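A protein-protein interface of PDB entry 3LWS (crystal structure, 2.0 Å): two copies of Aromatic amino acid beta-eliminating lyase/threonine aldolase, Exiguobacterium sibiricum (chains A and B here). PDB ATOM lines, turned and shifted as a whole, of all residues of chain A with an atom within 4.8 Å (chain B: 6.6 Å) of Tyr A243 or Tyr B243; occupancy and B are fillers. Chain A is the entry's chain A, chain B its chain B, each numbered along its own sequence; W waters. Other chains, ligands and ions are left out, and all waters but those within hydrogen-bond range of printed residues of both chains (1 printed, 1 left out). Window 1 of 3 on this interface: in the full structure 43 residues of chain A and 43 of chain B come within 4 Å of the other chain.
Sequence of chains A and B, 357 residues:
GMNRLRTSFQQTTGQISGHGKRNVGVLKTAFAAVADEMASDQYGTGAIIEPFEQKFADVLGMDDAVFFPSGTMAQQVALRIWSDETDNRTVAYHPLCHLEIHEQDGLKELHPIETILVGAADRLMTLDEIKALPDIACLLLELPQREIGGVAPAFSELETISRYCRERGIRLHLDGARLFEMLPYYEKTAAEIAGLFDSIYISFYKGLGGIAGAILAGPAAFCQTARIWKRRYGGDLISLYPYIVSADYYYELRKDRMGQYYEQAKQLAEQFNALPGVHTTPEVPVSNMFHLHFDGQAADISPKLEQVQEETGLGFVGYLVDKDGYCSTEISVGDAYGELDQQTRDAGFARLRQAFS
O of Ser A239 lies within hydrogen-bond range of OH of Tyr B243, at 2.5 Å.
The backbone carbonyl oxygen (O) of Ser B239 lies within hydrogen-bond range of the side-chain hydroxyl (OH) of Tyr A243 (2.7 Å).
O of Pro A242 lies within hydrogen-bond range of OG of Ser A246.
The backbone NH of Gly B213 is in hydrogen-bond range of the backbone carbonyl oxygen of Pro B69.
OG of Ser B246 sits at hydrogen-bond distance from O of Pro B242.
OG of Ser B246 sits at hydrogen-bond distance from O of Tyr B243, 3.0 Å away.
The backbone carbonyl oxygen of Tyr A243 lies within hydrogen-bond range of the side-chain hydroxyl of Ser A246 (3.2 Å).
Ser B239 touches Ile A211 (CB to CG2, 3.8 Å).
Tyr B241 touches Ile A211.
Pro B69 touches Leu A237.
CD2 of Leu A237 touches OH of Tyr B243, at 3.4 Å.
CB of Ser A239 touches CG2 of Ile B211 (3.5 Å).
OH of Tyr B243 touches CD2 of Leu A240 (3.5 Å).
CB of Leu B27 touches OH of Tyr A241, 3.8 Å away.
OH of Tyr A243 touches CD2 of Leu B237 (3.7 Å).
Leu B240 touches Tyr A243 (CA to OH, 3.5 Å).
OH of Tyr A243 touches CD of Pro B242, at 3.9 Å.
Printed residues of chain B within 4 Å of Leu A237: Pro B69 (3.4 Å) and Tyr B243 (3.4 Å).
Tyr A243 touches just these residues of chain B: Leu B237, Ser B239, Leu B240, Pro B242 and Tyr B243.
Phe B52 touches none of the printed residues of chain A.
Printed residues of chain A within 4 Å of Pro B69: Leu A237.
Of the printed residues of chain A, Ser B239 touches Ile A211 (3.8 Å) and Tyr A243 (2.7 Å).
Of chain A, only Leu A237 (3.4 Å), Ser A239 (2.5 Å), Leu A240 (3.5 Å) and Tyr A243 (3.4 Å) come within 4 Å of Tyr B243.
The nearest residue of chain B that does not touch Tyr A243 is Tyr B241 (4.9 Å).
The nearest residue of chain A that does not touch Tyr B243 is Pro A242 (4.2 Å).
Of the 13 printed residues of chain A, 7 touch a printed residue of chain B.
Hydrophobic or aromatic side chains of chain B that line the printed part of chain A: Leu B27, Ile B211, Leu B237, Leu B240, Tyr B241, Pro B242 and Tyr B243.
Among the printed residues, 15 pairs touch across the chains.
Among the printed residues, no Asp or Glu carboxylate lies within 4 Å of a Lys or Arg side-chain nitrogen of the other chain.
Ile A211 touches Ser B239, and with the chains exchanged Ser A239 touches Ile B211.
Ile A211 touches Tyr B241, and with the chains exchanged Tyr A241 touches Ile B211.
Leu A237 touches Tyr B243, and with the chains exchanged Tyr A243 touches Leu B237.
Leu A240 touches Tyr B243, and with the chains exchanged Tyr A243 touches Leu B240.
13 positions are printed for both chains.
Of the 15 pairs that touch across the chains among the printed residues, 11 have their exchanged pair printed and touching as well.
Water W1 lies within hydrogen-bond range of the backbone carbonyl oxygen (O) of Ile B211 (2.6 Å) and the side-chain hydroxyl (OG) of Ser A239 (3.0 Å).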
ATOM      1  N   PHE A  67       8.101  20.320  15.759  1.00  0.00           N
ATOM      2  CA  PHE A  67       9.211  20.625  14.882  1.00  0.00           C
ATOM      3  C   PHE A  67       9.595  22.092  15.046  1.00  0.00           C
ATOM      4  O   PHE A  67       8.770  22.960  14.854  1.00  0.00           O
ATOM      5  CB  PHE A  67       8.869  20.371  13.400  1.00  0.00           C
ATOM      6  CG  PHE A  67      10.087  20.422  12.496  1.00  0.00           C
ATOM      7  CD1 PHE A  67      10.868  19.292  12.308  1.00  0.00           C
ATOM      8  CD2 PHE A  67      10.452  21.585  11.869  1.00  0.00           C
ATOM      9  CE1 PHE A  67      12.017  19.336  11.508  1.00  0.00           C
ATOM     10  CE2 PHE A  67      11.574  21.634  11.054  1.00  0.00           C
ATOM     11  CZ  PHE A  67      12.347  20.511  10.865  1.00  0.00           C
ATOM     12  N   ILE A 211      20.012  19.311   6.870  1.00  0.00           N
ATOM     13  CA  ILE A 211      20.334  20.716   6.597  1.00  0.00           C
ATOM     14  C   ILE A 211      20.174  21.600   7.823  1.00  0.00           C
ATOM     15  O   ILE A 211      21.042  22.437   8.142  1.00  0.00           O
ATOM     16  CB  ILE A 211      19.459  21.221   5.458  1.00  0.00           C
ATOM     17  CG1 ILE A 211      19.890  20.487   4.174  1.00  0.00           C
ATOM     18  CG2 ILE A 211      19.585  22.757   5.281  1.00  0.00           C
ATOM     19  CD1 ILE A 211      18.948  20.689   2.979  1.00  0.00           C
ATOM     20  N   ALA A 212      19.065  21.415   8.513  1.00  0.00           N
ATOM     21  CA  ALA A 212      18.831  22.145   9.721  1.00  0.00           C
ATOM     22  C   ALA A 212      17.552  21.631  10.344  1.00  0.00           C
ATOM     23  O   ALA A 212      16.903  20.731   9.780  1.00  0.00           O
ATOM     24  CB  ALA A 212      18.752  23.670   9.405  1.00  0.00           C
ATOM     25  N   LEU A 237       6.885  29.258  10.883  1.00  0.00           N
ATOM     26  CA  LEU A 237       6.920  29.699   9.509  1.00  0.00           C
ATOM     27  C   LEU A 237       5.704  29.088   8.808  1.00  0.00           C
ATOM     28  O   LEU A 237       5.249  27.992   9.166  1.00  0.00           O
ATOM     29  CB  LEU A 237       8.234  29.273   8.817  1.00  0.00           C
ATOM     30  CG  LEU A 237       9.394  30.274   8.974  1.00  0.00           C
ATOM     31  CD1 LEU A 237       9.651  30.661  10.424  1.00  0.00           C
ATOM     32  CD2 LEU A 237      10.703  29.801   8.308  1.00  0.00           C
ATOM     33  N   SER A 239       5.797  27.697   6.007  1.00  0.00           N
ATOM     34  CA  SER A 239       6.299  26.472   5.352  1.00  0.00           C
ATOM     35  C   SER A 239       7.691  26.075   5.912  1.00  0.00           C
ATOM     36  O   SER A 239       8.676  26.745   5.666  1.00  0.00           O
ATOM     37  CB  SER A 239       6.416  26.667   3.826  1.00  0.00           C
ATOM     38  OG  SER A 239       5.176  26.821   3.174  1.00  0.00           O
ATOM     39  N   LEU A 240       7.727  25.020   6.716  1.00  0.00           N
ATOM     40  CA  LEU A 240       8.949  24.427   7.212  1.00  0.00           C
ATOM     41  C   LEU A 240       9.266  23.086   6.536  1.00  0.00           C
ATOM     42  O   LEU A 240      10.203  22.403   6.978  1.00  0.00           O
ATOM     43  CB  LEU A 240       8.871  24.237   8.729  1.00  0.00           C
ATOM     44  CG  LEU A 240       9.046  25.443   9.634  1.00  0.00           C
ATOM     45  CD1 LEU A 240       8.837  25.024  11.088  1.00  0.00           C
ATOM     46  CD2 LEU A 240      10.403  26.093   9.493  1.00  0.00           C
ATOM     47  N   TYR A 241       8.508  22.700   5.491  1.00  0.00           N
ATOM     48  CA  TYR A 241       8.796  21.440   4.789  1.00  0.00           C
ATOM     49  C   TYR A 241      10.235  21.351   4.245  1.00  0.00           C
ATOM     50  O   TYR A 241      10.829  20.286   4.334  1.00  0.00           O
ATOM     51  CB  TYR A 241       7.776  21.109   3.662  1.00  0.00           C
ATOM     52  CG  TYR A 241       7.777  22.020   2.445  1.00  0.00           C
ATOM     53  CD1 TYR A 241       8.613  21.775   1.342  1.00  0.00           C
ATOM     54  CD2 TYR A 241       6.921  23.102   2.368  1.00  0.00           C
ATOM     55  CE1 TYR A 241       8.628  22.625   0.235  1.00  0.00           C
ATOM     56  CE2 TYR A 241       6.895  23.925   1.244  1.00  0.00           C
ATOM     57  CZ  TYR A 241       7.747  23.677   0.192  1.00  0.00           C
ATOM     58  OH  TYR A 241       7.684  24.480  -0.896  1.00  0.00           O
ATOM     59  N   PRO A 242      10.812  22.466   3.729  1.00  0.00           N
ATOM     60  CA  PRO A 242      12.151  22.298   3.181  1.00  0.00           C
ATOM     61  C   PRO A 242      13.142  21.674   4.180  1.00  0.00           C
ATOM     62  O   PRO A 242      14.047  20.919   3.763  1.00  0.00           O
ATOM     63  CB  PRO A 242      12.553  23.727   2.772  1.00  0.00           C
ATOM     64  CG  PRO A 242      11.290  24.429   2.553  1.00  0.00           C
ATOM     65  CD  PRO A 242      10.392  23.880   3.659  1.00  0.00           C
ATOM     66  N   TYR A 243      12.941  21.950   5.475  1.00  0.00           N
ATOM     67  CA  TYR A 243      13.716  21.292   6.497  1.00  0.00           C
ATOM     68  C   TYR A 243      13.122  19.994   6.973  1.00  0.00           C
ATOM     69  O   TYR A 243      13.883  19.149   7.380  1.00  0.00           O
ATOM     70  CB  TYR A 243      13.939  22.172   7.709  1.00  0.00           C
ATOM     71  CG  TYR A 243      14.655  23.437   7.381  1.00  0.00           C
ATOM     72  CD1 TYR A 243      15.967  23.429   6.921  1.00  0.00           C
ATOM     73  CD2 TYR A 243      14.039  24.658   7.557  1.00  0.00           C
ATOM     74  CE1 TYR A 243      16.632  24.616   6.626  1.00  0.00           C
ATOM     75  CE2 TYR A 243      14.703  25.841   7.282  1.00  0.00           C
ATOM     76  CZ  TYR A 243      15.987  25.817   6.805  1.00  0.00           C
ATOM     77  OH  TYR A 243      16.647  27.013   6.538  1.00  0.00           O
ATOM     78  N   ILE A 244      11.796  19.819   6.928  1.00  0.00           N
ATOM     79  CA  ILE A 244      11.194  18.569   7.438  1.00  0.00           C
ATOM     80  C   ILE A 244      11.391  17.383   6.501  1.00  0.00           C
ATOM     81  O   ILE A 244      11.700  16.280   6.943  1.00  0.00           O
ATOM     82  CB  ILE A 244       9.686  18.736   7.766  1.00  0.00           C
ATOM     83  CG1 ILE A 244       9.489  19.764   8.876  1.00  0.00           C
ATOM     84  CG2 ILE A 244       9.061  17.439   8.264  1.00  0.00           C
ATOM     85  CD1 ILE A 244       8.078  20.197   8.994  1.00  0.00           C
ATOM     86  N   VAL A 245      11.214  17.609   5.215  1.00  0.00           N
ATOM     87  CA  VAL A 245      11.365  16.557   4.206  1.00  0.00           C
ATOM     88  C   VAL A 245      12.835  16.095   4.195  1.00  0.00           C
ATOM     89  O   VAL A 245      13.136  14.884   4.216  1.00  0.00           O
ATOM     90  CB  VAL A 245      11.026  17.116   2.818  1.00  0.00           C
ATOM     91  CG1 VAL A 245      11.461  16.156   1.719  1.00  0.00           C
ATOM     92  CG2 VAL A 245       9.508  17.539   2.709  1.00  0.00           C
ATOM     93  N   SER A 246      13.744  17.076   4.157  1.00  0.00           N
ATOM     94  CA  SER A 246      15.177  16.775   4.183  1.00  0.00           C
ATOM     95  C   SER A 246      15.563  16.063   5.471  1.00  0.00           C
ATOM     96  O   SER A 246      16.229  15.028   5.408  1.00  0.00           O
ATOM     97  CB  SER A 246      16.035  18.004   3.916  1.00  0.00           C
ATOM     98  OG  SER A 246      15.728  19.103   4.774  1.00  0.00           O
ATOM     99  N   ALA A 247      15.080  16.561   6.623  1.00  0.00           N
ATOM    100  CA  ALA A 247      15.322  15.941   7.936  1.00  0.00           C
ATOM    101  C   ALA A 247      14.935  14.477   7.972  1.00  0.00           C
ATOM    102  O   ALA A 247      15.726  13.607   8.368  1.00  0.00           O
ATOM    103  CB  ALA A 247      14.534  16.711   9.028  1.00  0.00           C
ATOM    104  N   LEU B  27       9.406  24.811  -4.336  1.00  0.00           N
ATOM    105  CA  LEU B  27      10.822  24.741  -3.920  1.00  0.00           C
ATOM    106  C   LEU B  27      11.658  24.171  -5.057  1.00  0.00           C
ATOM    107  O   LEU B  27      12.656  24.756  -5.433  1.00  0.00           O
ATOM    108  CB  LEU B  27      11.012  23.894  -2.662  1.00  0.00           C
ATOM    109  CG  LEU B  27      12.457  23.719  -2.133  1.00  0.00           C
ATOM    110  CD1 LEU B  27      13.071  25.069  -1.678  1.00  0.00           C
ATOM    111  CD2 LEU B  27      12.486  22.691  -1.002  1.00  0.00           C
ATOM    112  N   PHE B  31      14.944  25.735  -7.315  1.00  0.00           N
ATOM    113  CA  PHE B  31      16.247  25.100  -7.253  1.00  0.00           C
ATOM    114  C   PHE B  31      16.660  24.414  -8.600  1.00  0.00           C
ATOM    115  O   PHE B  31      17.816  23.998  -8.723  1.00  0.00           O
ATOM    116  CB  PHE B  31      16.332  24.111  -6.063  1.00  0.00           C
ATOM    117  CG  PHE B  31      16.680  24.788  -4.742  1.00  0.00           C
ATOM    118  CD1 PHE B  31      15.712  25.427  -3.979  1.00  0.00           C
ATOM    119  CD2 PHE B  31      17.988  24.854  -4.325  1.00  0.00           C
ATOM    120  CE1 PHE B  31      16.058  26.075  -2.804  1.00  0.00           C
ATOM    121  CE2 PHE B  31      18.357  25.523  -3.151  1.00  0.00           C
ATOM    122  CZ  PHE B  31      17.404  26.125  -2.384  1.00  0.00           C
ATOM    123  N   PHE B  52      22.764  38.083  -1.109  1.00  0.00           N
ATOM    124  CA  PHE B  52      21.367  38.397  -0.963  1.00  0.00           C
ATOM    125  C   PHE B  52      21.121  39.628  -0.092  1.00  0.00           C
ATOM    126  O   PHE B  52      20.385  40.547  -0.488  1.00  0.00           O
ATOM    127  CB  PHE B  52      20.613  37.171  -0.435  1.00  0.00           C
ATOM    128  CG  PHE B  52      19.134  37.311  -0.511  1.00  0.00           C
ATOM    129  CD1 PHE B  52      18.446  37.934   0.507  1.00  0.00           C
ATOM    130  CD2 PHE B  52      18.436  36.838  -1.605  1.00  0.00           C
ATOM    131  CE1 PHE B  52      17.050  38.090   0.445  1.00  0.00           C
ATOM    132  CE2 PHE B  52      17.035  36.974  -1.678  1.00  0.00           C
ATOM    133  CZ  PHE B  52      16.348  37.602  -0.646  1.00  0.00           C
ATOM    134  N   PHE B  67      18.880  38.775   6.562  1.00  0.00           N
ATOM    135  CA  PHE B  67      17.879  37.791   6.274  1.00  0.00           C
ATOM    136  C   PHE B  67      17.339  37.100   7.517  1.00  0.00           C
ATOM    137  O   PHE B  67      18.100  36.517   8.307  1.00  0.00           O
ATOM    138  CB  PHE B  67      18.414  36.737   5.298  1.00  0.00           C
ATOM    139  CG  PHE B  67      17.329  35.942   4.635  1.00  0.00           C
ATOM    140  CD1 PHE B  67      16.695  36.426   3.500  1.00  0.00           C
ATOM    141  CD2 PHE B  67      16.922  34.723   5.163  1.00  0.00           C
ATOM    142  CE1 PHE B  67      15.699  35.672   2.890  1.00  0.00           C
ATOM    143  CE2 PHE B  67      15.928  34.000   4.578  1.00  0.00           C
ATOM    144  CZ  PHE B  67      15.320  34.449   3.452  1.00  0.00           C
ATOM    145  N   PHE B  68      16.021  37.129   7.674  1.00  0.00           N
ATOM    146  CA  PHE B  68      15.360  36.470   8.813  1.00  0.00           C
ATOM    147  C   PHE B  68      14.495  35.333   8.290  1.00  0.00           C
ATOM    148  O   PHE B  68      13.971  35.424   7.167  1.00  0.00           O
ATOM    149  CB  PHE B  68      14.532  37.470   9.613  1.00  0.00           C
ATOM    150  CG  PHE B  68      15.329  38.245  10.642  1.00  0.00           C
ATOM    151  CD1 PHE B  68      16.036  39.379  10.290  1.00  0.00           C
ATOM    152  CD2 PHE B  68      15.340  37.851  11.965  1.00  0.00           C
ATOM    153  CE1 PHE B  68      16.765  40.070  11.238  1.00  0.00           C
ATOM    154  CE2 PHE B  68      16.060  38.546  12.918  1.00  0.00           C
ATOM    155  CZ  PHE B  68      16.768  39.653  12.552  1.00  0.00           C
ATOM    156  N   PRO B  69      14.359  34.251   9.087  1.00  0.00           N
ATOM    157  CA  PRO B  69      13.377  33.200   8.745  1.00  0.00           C
ATOM    158  C   PRO B  69      11.949  33.725   8.670  1.00  0.00           C
ATOM    159  O   PRO B  69      11.141  33.175   7.912  1.00  0.00           O
ATOM    160  CB  PRO B  69      13.512  32.186   9.874  1.00  0.00           C
ATOM    161  CG  PRO B  69      14.211  32.897  10.983  1.00  0.00           C
ATOM    162  CD  PRO B  69      14.977  34.026  10.402  1.00  0.00           C
ATOM    163  N   PHE B 204       9.162  37.702   1.546  1.00  0.00           N
ATOM    164  CA  PHE B 204       9.328  36.958   0.297  1.00  0.00           C
ATOM    165  C   PHE B 204       8.266  35.911   0.065  1.00  0.00           C
ATOM    166  O   PHE B 204       8.348  35.151  -0.911  1.00  0.00           O
ATOM    167  CB  PHE B 204      10.762  36.406   0.213  1.00  0.00           C
ATOM    168  CG  PHE B 204      11.772  37.511   0.121  1.00  0.00           C
ATOM    169  CD1 PHE B 204      12.004  38.144  -1.084  1.00  0.00           C
ATOM    170  CD2 PHE B 204      12.379  38.024   1.276  1.00  0.00           C
ATOM    171  CE1 PHE B 204      12.869  39.237  -1.152  1.00  0.00           C
ATOM    172  CE2 PHE B 204      13.249  39.091   1.199  1.00  0.00           C
ATOM    173  CZ  PHE B 204      13.509  39.689  -0.009  1.00  0.00           C
ATOM    174  N   ILE B 211       8.476  31.077  -0.520  1.00  0.00           N
ATOM    175  CA  ILE B 211       8.097  30.070   0.431  1.00  0.00           C
ATOM    176  C   ILE B 211       8.015  30.667   1.820  1.00  0.00           C
ATOM    177  O   ILE B 211       7.015  30.479   2.492  1.00  0.00           O
ATOM    178  CB  ILE B 211       9.056  28.895   0.388  1.00  0.00           C
ATOM    179  CG1 ILE B 211       9.024  28.256  -1.011  1.00  0.00           C
ATOM    180  CG2 ILE B 211       8.667  27.827   1.407  1.00  0.00           C
ATOM    181  CD1 ILE B 211       9.737  26.880  -1.076  1.00  0.00           C
ATOM    182  N   ALA B 212       9.058  31.393   2.222  1.00  0.00           N
ATOM    183  CA  ALA B 212       9.171  31.966   3.572  1.00  0.00           C
ATOM    184  C   ALA B 212      10.375  32.876   3.565  1.00  0.00           C
ATOM    185  O   ALA B 212      11.153  32.851   2.577  1.00  0.00           O
ATOM    186  CB  ALA B 212       9.369  30.847   4.659  1.00  0.00           C
ATOM    187  N   GLY B 213      10.524  33.691   4.622  1.00  0.00           N
ATOM    188  CA  GLY B 213      11.704  34.530   4.775  1.00  0.00           C
ATOM    189  C   GLY B 213      11.446  36.020   4.671  1.00  0.00           C
ATOM    190  O   GLY B 213      10.412  36.469   4.163  1.00  0.00           O
ATOM    191  N   LEU B 237      20.169  30.139  11.687  1.00  0.00           N
ATOM    192  CA  LEU B 237      20.249  28.736  11.361  1.00  0.00           C
ATOM    193  C   LEU B 237      21.545  28.510  10.585  1.00  0.00           C
ATOM    194  O   LEU B 237      22.033  29.404   9.866  1.00  0.00           O
ATOM    195  CB  LEU B 237      19.015  28.314  10.541  1.00  0.00           C
ATOM    196  CG  LEU B 237      17.716  27.896  11.228  1.00  0.00           C
ATOM    197  CD1 LEU B 237      17.358  28.813  12.357  1.00  0.00           C
ATOM    198  CD2 LEU B 237      16.596  27.829  10.174  1.00  0.00           C
ATOM    199  N   SER B 239      21.969  26.891   8.026  1.00  0.00           N
ATOM    200  CA  SER B 239      21.708  27.024   6.597  1.00  0.00           C
ATOM    201  C   SER B 239      20.322  27.559   6.355  1.00  0.00           C
ATOM    202  O   SER B 239      19.351  26.822   6.523  1.00  0.00           O
ATOM    203  CB  SER B 239      21.876  25.667   5.891  1.00  0.00           C
ATOM    204  OG  SER B 239      23.223  25.218   5.964  1.00  0.00           O
ATOM    205  N   LEU B 240      20.230  28.842   5.999  1.00  0.00           N
ATOM    206  CA  LEU B 240      18.960  29.429   5.525  1.00  0.00           C
ATOM    207  C   LEU B 240      18.761  29.427   3.999  1.00  0.00           C
ATOM    208  O   LEU B 240      17.695  29.832   3.551  1.00  0.00           O
ATOM    209  CB  LEU B 240      18.779  30.857   6.084  1.00  0.00           C
ATOM    210  CG  LEU B 240      18.453  30.937   7.560  1.00  0.00           C
ATOM    211  CD1 LEU B 240      18.593  32.382   8.058  1.00  0.00           C
ATOM    212  CD2 LEU B 240      17.040  30.369   7.834  1.00  0.00           C
ATOM    213  N   TYR B 241      19.746  28.962   3.208  1.00  0.00           N
ATOM    214  CA  TYR B 241      19.633  28.952   1.718  1.00  0.00           C
ATOM    215  C   TYR B 241      18.361  28.354   1.127  1.00  0.00           C
ATOM    216  O   TYR B 241      17.937  28.825   0.092  1.00  0.00           O
ATOM    217  CB  TYR B 241      20.823  28.260   1.010  1.00  0.00           C
ATOM    218  CG  TYR B 241      20.863  26.756   1.146  1.00  0.00           C
ATOM    219  CD1 TYR B 241      20.195  25.912   0.256  1.00  0.00           C
ATOM    220  CD2 TYR B 241      21.646  26.170   2.127  1.00  0.00           C
ATOM    221  CE1 TYR B 241      20.260  24.525   0.407  1.00  0.00           C
ATOM    222  CE2 TYR B 241      21.720  24.829   2.286  1.00  0.00           C
ATOM    223  CZ  TYR B 241      21.040  23.988   1.419  1.00  0.00           C
ATOM    224  OH  TYR B 241      21.154  22.639   1.659  1.00  0.00           O
ATOM    225  N   PRO B 242      17.735  27.340   1.771  1.00  0.00           N
ATOM    226  CA  PRO B 242      16.490  26.930   1.122  1.00  0.00           C
ATOM    227  C   PRO B 242      15.468  28.063   0.950  1.00  0.00           C
ATOM    228  O   PRO B 242      14.713  28.061  -0.026  1.00  0.00           O
ATOM    229  CB  PRO B 242      15.968  25.835   2.020  1.00  0.00           C
ATOM    230  CG  PRO B 242      17.147  25.352   2.747  1.00  0.00           C
ATOM    231  CD  PRO B 242      18.012  26.510   2.954  1.00  0.00           C
ATOM    232  N   TYR B 243      15.451  29.009   1.881  1.00  0.00           N
ATOM    233  CA  TYR B 243      14.569  30.159   1.797  1.00  0.00           C
ATOM    234  C   TYR B 243      15.145  31.290   0.993  1.00  0.00           C
ATOM    235  O   TYR B 243      14.421  31.954   0.233  1.00  0.00           O
ATOM    236  CB  TYR B 243      14.209  30.690   3.208  1.00  0.00           C
ATOM    237  CG  TYR B 243      13.377  29.724   4.001  1.00  0.00           C
ATOM    238  CD1 TYR B 243      12.262  29.122   3.458  1.00  0.00           C
ATOM    239  CD2 TYR B 243      13.713  29.410   5.297  1.00  0.00           C
ATOM    240  CE1 TYR B 243      11.500  28.257   4.193  1.00  0.00           C
ATOM    241  CE2 TYR B 243      12.969  28.540   6.026  1.00  0.00           C
ATOM    242  CZ  TYR B 243      11.856  27.968   5.479  1.00  0.00           C
ATOM    243  OH  TYR B 243      11.115  27.107   6.243  1.00  0.00           O
ATOM    244  N   ILE B 244      16.438  31.508   1.156  1.00  0.00           N
ATOM    245  CA  ILE B 244      17.118  32.619   0.503  1.00  0.00           C
ATOM    246  C   ILE B 244      17.069  32.461  -1.017  1.00  0.00           C
ATOM    247  O   ILE B 244      16.672  33.405  -1.747  1.00  0.00           O
ATOM    248  CB  ILE B 244      18.576  32.671   0.901  1.00  0.00           C
ATOM    249  CG1 ILE B 244      18.707  32.926   2.415  1.00  0.00           C
ATOM    250  CG2 ILE B 244      19.283  33.768   0.067  1.00  0.00           C
ATOM    251  CD1 ILE B 244      20.110  32.634   2.920  1.00  0.00           C
ATOM    252  N   VAL B 245      17.465  31.265  -1.463  1.00  0.00           N
ATOM    253  CA  VAL B 245      17.565  30.954  -2.894  1.00  0.00           C
ATOM    254  C   VAL B 245      16.153  30.999  -3.514  1.00  0.00           C
ATOM    255  O   VAL B 245      15.914  31.614  -4.555  1.00  0.00           O
ATOM    256  CB  VAL B 245      18.242  29.563  -3.142  1.00  0.00           C
ATOM    257  CG1 VAL B 245      18.218  29.233  -4.597  1.00  0.00           C
ATOM    258  CG2 VAL B 245      19.716  29.519  -2.645  1.00  0.00           C
ATOM    259  N   SER B 246      15.198  30.395  -2.829  1.00  0.00           N
ATOM    260  CA  SER B 246      13.834  30.471  -3.257  1.00  0.00           C
ATOM    261  C   SER B 246      13.304  31.906  -3.226  1.00  0.00           C
ATOM    262  O   SER B 246      12.674  32.320  -4.189  1.00  0.00           O
ATOM    263  CB  SER B 246      12.970  29.480  -2.482  1.00  0.00           C
ATOM    264  OG  SER B 246      12.858  29.834  -1.127  1.00  0.00           O
ATOM    265  N   ALA B 247      13.579  32.689  -2.169  1.00  0.00           N
ATOM    266  CA  ALA B 247      13.181  34.098  -2.141  1.00  0.00           C
ATOM    267  C   ALA B 247      13.670  34.811  -3.422  1.00  0.00           C
ATOM    268  O   ALA B 247      12.878  35.373  -4.160  1.00  0.00           O
ATOM    269  CB  ALA B 247      13.740  34.833  -0.839  1.00  0.00           C
ATOM    270  N   ASP B 248      14.962  34.691  -3.727  1.00  0.00           N
ATOM    271  CA  ASP B 248      15.563  35.338  -4.922  1.00  0.00           C
ATOM    272  C   ASP B 248      14.906  34.879  -6.211  1.00  0.00           C
ATOM    273  O   ASP B 248      14.604  35.696  -7.071  1.00  0.00           O
ATOM    274  CB  ASP B 248      17.069  35.023  -5.004  1.00  0.00           C
ATOM    275  CG  ASP B 248      17.927  36.234  -5.342  1.00  0.00           C
ATOM    276  OD1 ASP B 248      17.402  37.358  -5.595  1.00  0.00           O
ATOM    277  OD2 ASP B 248      19.174  36.059  -5.283  1.00  0.00           O
HETATM  278  O   HOH W   1       4.914  29.242   1.508  1.00  0.00           O
